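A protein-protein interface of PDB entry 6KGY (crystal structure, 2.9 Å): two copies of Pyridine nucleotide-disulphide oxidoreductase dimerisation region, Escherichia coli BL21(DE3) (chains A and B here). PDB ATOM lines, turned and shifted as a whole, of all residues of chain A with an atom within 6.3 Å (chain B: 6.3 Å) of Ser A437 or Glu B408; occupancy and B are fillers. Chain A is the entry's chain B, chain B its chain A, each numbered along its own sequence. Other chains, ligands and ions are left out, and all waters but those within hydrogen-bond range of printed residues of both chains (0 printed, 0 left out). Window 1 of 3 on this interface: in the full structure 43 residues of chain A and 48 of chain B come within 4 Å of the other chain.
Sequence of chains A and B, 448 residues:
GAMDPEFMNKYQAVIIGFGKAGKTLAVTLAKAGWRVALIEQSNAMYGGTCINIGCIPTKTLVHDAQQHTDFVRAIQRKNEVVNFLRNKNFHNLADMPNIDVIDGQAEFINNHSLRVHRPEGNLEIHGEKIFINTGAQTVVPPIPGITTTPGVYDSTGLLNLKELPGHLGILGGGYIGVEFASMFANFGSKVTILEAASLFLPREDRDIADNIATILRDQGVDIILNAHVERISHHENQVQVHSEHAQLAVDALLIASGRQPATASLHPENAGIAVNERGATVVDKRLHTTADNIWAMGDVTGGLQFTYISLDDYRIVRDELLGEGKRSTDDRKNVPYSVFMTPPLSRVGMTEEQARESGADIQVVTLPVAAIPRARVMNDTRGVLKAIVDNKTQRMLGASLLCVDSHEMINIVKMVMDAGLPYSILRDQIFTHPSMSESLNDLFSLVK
Of the printed residues of chain B, Met A409 touches Glu B408.
Of the printed residues of chain B, Ser A435 touches His B407 and Glu B408.
Of the printed residues of chain B, Met A436 touches Glu B408.
Ser A437 touches two residues of chain B.
Printed residues of chain A within 4 Å of His B407: Arg A374 (2.9 Å), Thr A432 (3.9 Å), Pro A434 (3.99 Å) and Ser A435 (3.96 Å).
Of chain A, only Met A409 (3.5 Å), Ser A435 (3.1 Å), Met A436 (2.7 Å) and Ser A437 (2.7 Å) come within 4 Å of Glu B408.
Of the printed residues of chain A, Ile B412 touches Ile A412.
The nearest residue of chain B that does not touch Ser A437 is His B407 (5.4 Å).
The nearest printed residue of chain B that does not touch Thr A432 is Ser B346 (5.2 Å).
OG of Ser A437 sits close to ND2 of Asn B411 (3.4 Å).
NE2 of His B407 is in hydrogen-bond range of NH2 of Arg A374 (2.9 Å).
The side-chain carboxylate of Asp A405 lies close to the side-chain carboxylate of Asp B405, 3.1 Å away.
N of Met A436 sits at hydrogen-bond distance from OE1 of Glu B408 (2.7 Å).
OE2 of Glu B408 sits at hydrogen-bond distance from OG of Ser A437.
Of the 10 printed residues of chain B, 7 touch a printed residue of chain A.
Hydrophobic or aromatic side chains of chain B within 4 Å of the printed part of chain A: His B407, Ile B410 and Ile B412.
Of the 16 printed residues of chain A, 10 touch a printed residue of chain B.
Along chain A the printed residues that touch a printed residue of chain B span positions 374 to 437.
Among the printed residues, 16 pairs touch across the chains.
Among the printed residues, no Asp or Glu carboxylate lies within 4 Å of a Lys or Arg side-chain nitrogen of the other chain.
Met A409 touches Glu B408.
Asn B411 touches Ile A412 (C to CD1, 3.5 Å).
Ile B412 touches Ile A412.
Asn B411 touches Phe A431 (CG to CD1, 3.7 Å).
Ser B338 touches Thr A432 (OG to CG2, 3.3 Å).
Thr A432 touches Ile B410 (OG1 to CG2, 3.8 Å).
Asn B411 touches Thr A432.
CD2 of His B407 touches O of Pro A434, 3.99 Å away.
Ser A435 touches His B407 (CB to CD2, 3.96 Å).
Ser A435 touches Glu B408.
Asp B405 touches its own counterpart, Asp A405.
Met A409 touches Glu B408, but with the chains exchanged Glu A408 does not touch Met B409 (5.1 Å).
Ile B412 touches its own counterpart, Ile A412.
Positions printed for both chains: 405, 408, 409 and 412.
The side-chain amide nitrogen (ND2) of Asn B411 lies within hydrogen-bond range of the backbone carbonyl oxygen (O) of Glu B408 (3.4 Å).
The backbone carbonyl oxygen (O) of His B407 sits at hydrogen-bond distance from the side-chain amide nitrogen (ND2) of Asn B411 (3.2 Å).
OG of Ser B346 sits at hydrogen-bond distance from N of His B407, 3.0 Å away.
OG of Ser A435 sits at hydrogen-bond distance from O of Thr A432 (2.6 Å).
The side-chain hydroxyl of Ser B338 lies within hydrogen-bond range of the side-chain hydroxyl of Ser B346 (2.5 Å).
The backbone NH of Glu A438 lies within hydrogen-bond range of the side-chain hydroxyl of Ser A435, at 3.2 Å.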
ATOM      1  N   ARG A 374     -12.686  30.606 -35.106  1.00  0.00           N
ATOM      2  CA  ARG A 374     -11.633  31.203 -34.296  1.00  0.00           C
ATOM      3  C   ARG A 374     -10.250  30.990 -34.901  1.00  0.00           C
ATOM      4  O   ARG A 374      -9.340  31.783 -34.633  1.00  0.00           O
ATOM      5  CB  ARG A 374     -11.689  30.630 -32.880  1.00  0.00           C
ATOM      6  CG  ARG A 374     -10.723  31.268 -31.903  1.00  0.00           C
ATOM      7  CD  ARG A 374     -11.136  32.687 -31.554  1.00  0.00           C
ATOM      8  NE  ARG A 374      -9.980  33.563 -31.375  1.00  0.00           N
ATOM      9  CZ  ARG A 374      -9.127  33.481 -30.360  1.00  0.00           C
ATOM     10  NH1 ARG A 374      -8.103  34.321 -30.284  1.00  0.00           N
ATOM     11  NH2 ARG A 374      -9.291  32.561 -29.420  1.00  0.00           N
ATOM     12  N   VAL A 404      -4.336  25.563 -33.003  1.00  0.00           N
ATOM     13  CA  VAL A 404      -3.786  26.573 -32.107  1.00  0.00           C
ATOM     14  C   VAL A 404      -4.529  26.525 -30.782  1.00  0.00           C
ATOM     15  O   VAL A 404      -5.756  26.362 -30.738  1.00  0.00           O
ATOM     16  CB  VAL A 404      -3.868  27.972 -32.739  1.00  0.00           C
ATOM     17  CG1 VAL A 404      -2.713  28.194 -33.696  1.00  0.00           C
ATOM     18  CG2 VAL A 404      -5.194  28.157 -33.451  1.00  0.00           C
ATOM     19  N   ASP A 405      -3.777  26.657 -29.689  1.00  0.00           N
ATOM     20  CA  ASP A 405      -4.325  26.630 -28.333  1.00  0.00           C
ATOM     21  C   ASP A 405      -5.034  25.313 -28.028  1.00  0.00           C
ATOM     22  O   ASP A 405      -6.034  25.286 -27.306  1.00  0.00           O
ATOM     23  CB  ASP A 405      -5.267  27.814 -28.089  1.00  0.00           C
ATOM     24  CG  ASP A 405      -4.522  29.088 -27.753  1.00  0.00           C
ATOM     25  OD1 ASP A 405      -4.191  29.847 -28.688  1.00  0.00           O
ATOM     26  OD2 ASP A 405      -4.268  29.332 -26.555  1.00  0.00           O
ATOM     27  N   GLU A 408      -5.038  24.065 -24.237  1.00  0.00           N
ATOM     28  CA  GLU A 408      -6.072  24.521 -23.316  1.00  0.00           C
ATOM     29  C   GLU A 408      -7.364  23.727 -23.444  1.00  0.00           C
ATOM     30  O   GLU A 408      -8.044  23.494 -22.440  1.00  0.00           O
ATOM     31  CB  GLU A 408      -6.365  26.008 -23.539  1.00  0.00           C
ATOM     32  CG  GLU A 408      -5.126  26.887 -23.617  1.00  0.00           C
ATOM     33  CD  GLU A 408      -4.544  27.199 -22.253  1.00  0.00           C
ATOM     34  OE1 GLU A 408      -5.193  26.873 -21.237  1.00  0.00           O
ATOM     35  OE2 GLU A 408      -3.433  27.767 -22.195  1.00  0.00           O
ATOM     36  N   MET A 409      -7.716  23.303 -24.661  1.00  0.00           N
ATOM     37  CA  MET A 409      -8.942  22.541 -24.863  1.00  0.00           C
ATOM     38  C   MET A 409      -8.800  21.090 -24.423  1.00  0.00           C
ATOM     39  O   MET A 409      -9.801  20.459 -24.065  1.00  0.00           O
ATOM     40  CB  MET A 409      -9.362  22.585 -26.333  1.00  0.00           C
ATOM     41  CG  MET A 409      -9.302  23.959 -26.970  1.00  0.00           C
ATOM     42  SD  MET A 409      -9.391  23.858 -28.769  1.00  0.00           S
ATOM     43  CE  MET A 409     -10.256  22.303 -28.988  1.00  0.00           C
ATOM     44  N   ILE A 412     -10.389  20.536 -21.042  1.00  0.00           N
ATOM     45  CA  ILE A 412     -11.839  20.368 -21.021  1.00  0.00           C
ATOM     46  C   ILE A 412     -12.202  18.917 -21.306  1.00  0.00           C
ATOM     47  O   ILE A 412     -13.066  18.333 -20.641  1.00  0.00           O
ATOM     48  CB  ILE A 412     -12.501  21.326 -22.028  1.00  0.00           C
ATOM     49  CG1 ILE A 412     -12.406  22.773 -21.541  1.00  0.00           C
ATOM     50  CG2 ILE A 412     -13.949  20.937 -22.264  1.00  0.00           C
ATOM     51  CD1 ILE A 412     -13.556  23.194 -20.653  1.00  0.00           C
ATOM     52  N   PHE A 431     -20.432  27.896 -24.463  1.00  0.00           N
ATOM     53  CA  PHE A 431     -19.022  28.249 -24.379  1.00  0.00           C
ATOM     54  C   PHE A 431     -18.871  29.772 -24.395  1.00  0.00           C
ATOM     55  O   PHE A 431     -19.807  30.512 -24.080  1.00  0.00           O
ATOM     56  CB  PHE A 431     -18.247  27.594 -25.525  1.00  0.00           C
ATOM     57  CG  PHE A 431     -17.996  26.128 -25.334  1.00  0.00           C
ATOM     58  CD1 PHE A 431     -17.045  25.684 -24.431  1.00  0.00           C
ATOM     59  CD2 PHE A 431     -18.699  25.191 -26.073  1.00  0.00           C
ATOM     60  CE1 PHE A 431     -16.808  24.334 -24.260  1.00  0.00           C
ATOM     61  CE2 PHE A 431     -18.466  23.841 -25.909  1.00  0.00           C
ATOM     62  CZ  PHE A 431     -17.519  23.410 -25.002  1.00  0.00           C
ATOM     63  N   THR A 432     -17.685  30.249 -24.757  1.00  0.00           N
ATOM     64  CA  THR A 432     -17.413  31.661 -24.974  1.00  0.00           C
ATOM     65  C   THR A 432     -17.094  31.875 -26.448  1.00  0.00           C
ATOM     66  O   THR A 432     -16.392  31.066 -27.061  1.00  0.00           O
ATOM     67  CB  THR A 432     -16.250  32.137 -24.094  1.00  0.00           C
ATOM     68  OG1 THR A 432     -16.704  32.287 -22.742  1.00  0.00           O
ATOM     69  CG2 THR A 432     -15.695  33.469 -24.584  1.00  0.00           C
ATOM     70  N   PRO A 434     -15.752  34.613 -29.556  1.00  0.00           N
ATOM     71  CA  PRO A 434     -15.212  33.487 -30.326  1.00  0.00           C
ATOM     72  C   PRO A 434     -14.040  32.828 -29.609  1.00  0.00           C
ATOM     73  O   PRO A 434     -13.180  33.530 -29.078  1.00  0.00           O
ATOM     74  CB  PRO A 434     -14.747  34.143 -31.638  1.00  0.00           C
ATOM     75  CG  PRO A 434     -15.077  35.629 -31.505  1.00  0.00           C
ATOM     76  CD  PRO A 434     -15.219  35.891 -30.046  1.00  0.00           C
ATOM     77  N   SER A 435     -13.994  31.498 -29.595  1.00  0.00           N
ATOM     78  CA  SER A 435     -12.952  30.799 -28.862  1.00  0.00           C
ATOM     79  C   SER A 435     -12.577  29.522 -29.597  1.00  0.00           C
ATOM     80  O   SER A 435     -13.231  29.113 -30.559  1.00  0.00           O
ATOM     81  CB  SER A 435     -13.395  30.483 -27.430  1.00  0.00           C
ATOM     82  OG  SER A 435     -14.406  29.490 -27.414  1.00  0.00           O
ATOM     83  N   MET A 436     -11.492  28.901 -29.135  1.00  0.00           N
ATOM     84  CA  MET A 436     -11.092  27.600 -29.652  1.00  0.00           C
ATOM     85  C   MET A 436     -11.930  26.477 -29.062  1.00  0.00           C
ATOM     86  O   MET A 436     -12.162  25.464 -29.731  1.00  0.00           O
ATOM     87  CB  MET A 436      -9.611  27.350 -29.359  1.00  0.00           C
ATOM     88  CG  MET A 436      -8.701  27.770 -30.481  1.00  0.00           C
ATOM     89  SD  MET A 436      -9.384  27.254 -32.060  1.00  0.00           S
ATOM     90  CE  MET A 436      -8.663  28.487 -33.119  1.00  0.00           C
ATOM     91  N   SER A 437     -12.396  26.645 -27.824  1.00  0.00           N
ATOM     92  CA  SER A 437     -13.128  25.594 -27.132  1.00  0.00           C
ATOM     93  C   SER A 437     -14.570  25.463 -27.606  1.00  0.00           C
ATOM     94  O   SER A 437     -15.158  24.387 -27.450  1.00  0.00           O
ATOM     95  CB  SER A 437     -13.106  25.851 -25.624  1.00  0.00           C
ATOM     96  OG  SER A 437     -11.823  26.282 -25.201  1.00  0.00           O
ATOM     97  N   GLU A 438     -15.152  26.521 -28.176  1.00  0.00           N
ATOM     98  CA  GLU A 438     -16.534  26.441 -28.636  1.00  0.00           C
ATOM     99  C   GLU A 438     -16.694  25.515 -29.834  1.00  0.00           C
ATOM    100  O   GLU A 438     -17.787  24.977 -30.040  1.00  0.00           O
ATOM    101  CB  GLU A 438     -17.063  27.831 -28.988  1.00  0.00           C
ATOM    102  CG  GLU A 438     -16.193  28.599 -29.956  1.00  0.00           C
ATOM    103  CD  GLU A 438     -16.993  29.462 -30.905  1.00  0.00           C
ATOM    104  OE1 GLU A 438     -18.203  29.649 -30.663  1.00  0.00           O
ATOM    105  OE2 GLU A 438     -16.411  29.956 -31.895  1.00  0.00           O
ATOM    106  N   SER A 439     -15.636  25.309 -30.624  1.00  0.00           N
ATOM    107  CA  SER A 439     -15.717  24.383 -31.750  1.00  0.00           C
ATOM    108  C   SER A 439     -15.803  22.928 -31.310  1.00  0.00           C
ATOM    109  O   SER A 439     -15.871  22.043 -32.171  1.00  0.00           O
ATOM    110  CB  SER A 439     -14.523  24.581 -32.683  1.00  0.00           C
ATOM    111  OG  SER A 439     -14.830  25.528 -33.691  1.00  0.00           O
ATOM    112  N   LEU A 440     -15.790  22.657 -30.005  1.00  0.00           N
ATOM    113  CA  LEU A 440     -16.140  21.333 -29.509  1.00  0.00           C
ATOM    114  C   LEU A 440     -17.643  21.095 -29.540  1.00  0.00           C
ATOM    115  O   LEU A 440     -18.074  19.937 -29.518  1.00  0.00           O
ATOM    116  CB  LEU A 440     -15.607  21.141 -28.088  1.00  0.00           C
ATOM    117  CG  LEU A 440     -14.129  20.757 -27.998  1.00  0.00           C
ATOM    118  CD1 LEU A 440     -13.585  21.007 -26.599  1.00  0.00           C
ATOM    119  CD2 LEU A 440     -13.930  19.306 -28.405  1.00  0.00           C
ATOM    120  N   ASN A 441     -18.442  22.164 -29.580  1.00  0.00           N
ATOM    121  CA  ASN A 441     -19.871  22.019 -29.839  1.00  0.00           C
ATOM    122  C   ASN A 441     -20.106  21.326 -31.175  1.00  0.00           C
ATOM    123  O   ASN A 441     -20.928  20.410 -31.281  1.00  0.00           O
ATOM    124  CB  ASN A 441     -20.550  23.391 -29.831  1.00  0.00           C
ATOM    125  CG  ASN A 441     -20.904  23.866 -28.438  1.00  0.00           C
ATOM    126  OD1 ASN A 441     -21.027  23.070 -27.508  1.00  0.00           O
ATOM    127  ND2 ASN A 441     -21.078  25.175 -28.288  1.00  0.00           N
ATOM    128  N   SER B 338     -17.138  37.411 -22.027  1.00  0.00           N
ATOM    129  CA  SER B 338     -15.746  37.808 -22.168  1.00  0.00           C
ATOM    130  C   SER B 338     -15.654  39.182 -22.814  1.00  0.00           C
ATOM    131  O   SER B 338     -16.356  39.468 -23.788  1.00  0.00           O
ATOM    132  CB  SER B 338     -14.959  36.791 -23.007  1.00  0.00           C
ATOM    133  OG  SER B 338     -14.722  35.600 -22.279  1.00  0.00           O
ATOM    134  N   SER B 346     -12.504  37.537 -18.766  1.00  0.00           N
ATOM    135  CA  SER B 346     -13.549  36.537 -18.928  1.00  0.00           C
ATOM    136  C   SER B 346     -14.174  36.261 -17.572  1.00  0.00           C
ATOM    137  O   SER B 346     -13.461  36.004 -16.598  1.00  0.00           O
ATOM    138  CB  SER B 346     -12.993  35.251 -19.537  1.00  0.00           C
ATOM    139  OG  SER B 346     -12.599  35.479 -20.877  1.00  0.00           O
ATOM    140  N   ASP B 405      -5.553  34.345 -22.706  1.00  0.00           N
ATOM    141  CA  ASP B 405      -6.380  33.173 -22.997  1.00  0.00           C
ATOM    142  C   ASP B 405      -7.419  32.918 -21.909  1.00  0.00           C
ATOM    143  O   ASP B 405      -7.835  31.777 -21.690  1.00  0.00           O
ATOM    144  CB  ASP B 405      -5.518  31.924 -23.213  1.00  0.00           C
ATOM    145  CG  ASP B 405      -4.632  32.033 -24.436  1.00  0.00           C
ATOM    146  OD1 ASP B 405      -3.511  31.484 -24.409  1.00  0.00           O
ATOM    147  OD2 ASP B 405      -5.056  32.668 -25.425  1.00  0.00           O
ATOM    148  N   SER B 406      -7.850  33.977 -21.218  1.00  0.00           N
ATOM    149  CA  SER B 406      -8.867  33.815 -20.185  1.00  0.00           C
ATOM    150  C   SER B 406     -10.193  33.355 -20.774  1.00  0.00           C
ATOM    151  O   SER B 406     -10.991  32.714 -20.081  1.00  0.00           O
ATOM    152  CB  SER B 406      -9.049  35.123 -19.416  1.00  0.00           C
ATOM    153  OG  SER B 406      -9.853  36.035 -20.141  1.00  0.00           O
ATOM    154  N   HIS B 407     -10.444  33.667 -22.049  1.00  0.00           N
ATOM    155  CA  HIS B 407     -11.655  33.187 -22.707  1.00  0.00           C
ATOM    156  C   HIS B 407     -11.646  31.672 -22.856  1.00  0.00           C
ATOM    157  O   HIS B 407     -12.704  31.037 -22.778  1.00  0.00           O
ATOM    158  CB  HIS B 407     -11.812  33.862 -24.069  1.00  0.00           C
ATOM    159  CG  HIS B 407     -10.655  33.637 -24.992  1.00  0.00           C
ATOM    160  ND1 HIS B 407      -9.411  34.191 -24.775  1.00  0.00           N
ATOM    161  CD2 HIS B 407     -10.552  32.917 -26.133  1.00  0.00           C
ATOM    162  CE1 HIS B 407      -8.592  33.821 -25.742  1.00  0.00           C
ATOM    163  NE2 HIS B 407      -9.260  33.048 -26.580  1.00  0.00           N
ATOM    164  N   GLU B 408     -10.470  31.079 -23.074  1.00  0.00           N
ATOM    165  CA  GLU B 408     -10.362  29.625 -23.066  1.00  0.00           C
ATOM    166  C   GLU B 408     -10.479  29.076 -21.650  1.00  0.00           C
ATOM    167  O   GLU B 408     -11.082  28.019 -21.432  1.00  0.00           O
ATOM    168  CB  GLU B 408      -9.033  29.194 -23.687  1.00  0.00           C
ATOM    169  CG  GLU B 408      -8.907  29.474 -25.172  1.00  0.00           C
ATOM    170  CD  GLU B 408      -9.793  28.576 -26.006  1.00  0.00           C
ATOM    171  OE1 GLU B 408     -10.769  29.085 -26.592  1.00  0.00           O
ATOM    172  OE2 GLU B 408      -9.516  27.360 -26.074  1.00  0.00           O
ATOM    173  N   MET B 409      -9.916  29.795 -20.676  1.00  0.00           N
ATOM    174  CA  MET B 409      -9.804  29.281 -19.315  1.00  0.00           C
ATOM    175  C   MET B 409     -11.167  29.134 -18.654  1.00  0.00           C
ATOM    176  O   MET B 409     -11.449  28.116 -18.011  1.00  0.00           O
ATOM    177  CB  MET B 409      -8.915  30.207 -18.488  1.00  0.00           C
ATOM    178  CG  MET B 409      -7.823  29.510 -17.707  1.00  0.00           C
ATOM    179  SD  MET B 409      -6.731  30.729 -16.962  1.00  0.00           S
ATOM    180  CE  MET B 409      -6.415  31.770 -18.383  1.00  0.00           C
ATOM    181  N   ILE B 410     -12.026  30.148 -18.795  1.00  0.00           N
ATOM    182  CA  ILE B 410     -13.281  30.192 -18.053  1.00  0.00           C
ATOM    183  C   ILE B 410     -14.193  29.020 -18.389  1.00  0.00           C
ATOM    184  O   ILE B 410     -15.077  28.681 -17.596  1.00  0.00           O
ATOM    185  CB  ILE B 410     -13.992  31.540 -18.303  1.00  0.00           C
ATOM    186  CG1 ILE B 410     -14.838  31.931 -17.089  1.00  0.00           C
ATOM    187  CG2 ILE B 410     -14.846  31.481 -19.561  1.00  0.00           C
ATOM    188  CD1 ILE B 410     -14.084  32.738 -16.057  1.00  0.00           C
ATOM    189  N   ASN B 411     -13.992  28.379 -19.544  1.00  0.00           N
ATOM    190  CA  ASN B 411     -14.823  27.237 -19.909  1.00  0.00           C
ATOM    191  C   ASN B 411     -14.616  26.076 -18.944  1.00  0.00           C
ATOM    192  O   ASN B 411     -15.560  25.341 -18.633  1.00  0.00           O
ATOM    193  CB  ASN B 411     -14.523  26.812 -21.346  1.00  0.00           C
ATOM    194  CG  ASN B 411     -14.853  27.896 -22.354  1.00  0.00           C
ATOM    195  OD1 ASN B 411     -15.906  28.531 -22.279  1.00  0.00           O
ATOM    196  ND2 ASN B 411     -13.950  28.118 -23.300  1.00  0.00           N
ATOM    197  N   ILE B 412     -13.384  25.895 -18.460  1.00  0.00           N
ATOM    198  CA  ILE B 412     -13.130  24.890 -17.433  1.00  0.00           C
ATOM    199  C   ILE B 412     -13.832  25.268 -16.137  1.00  0.00           C
ATOM    200  O   ILE B 412     -14.439  24.422 -15.470  1.00  0.00           O
ATOM    201  CB  ILE B 412     -11.615  24.717 -17.219  1.00  0.00           C
ATOM    202  CG1 ILE B 412     -10.923  24.343 -18.532  1.00  0.00           C
ATOM    203  CG2 ILE B 412     -11.344  23.672 -16.145  1.00  0.00           C
ATOM    204  CD1 ILE B 412      -9.482  23.922 -18.362  1.00  0.00           C
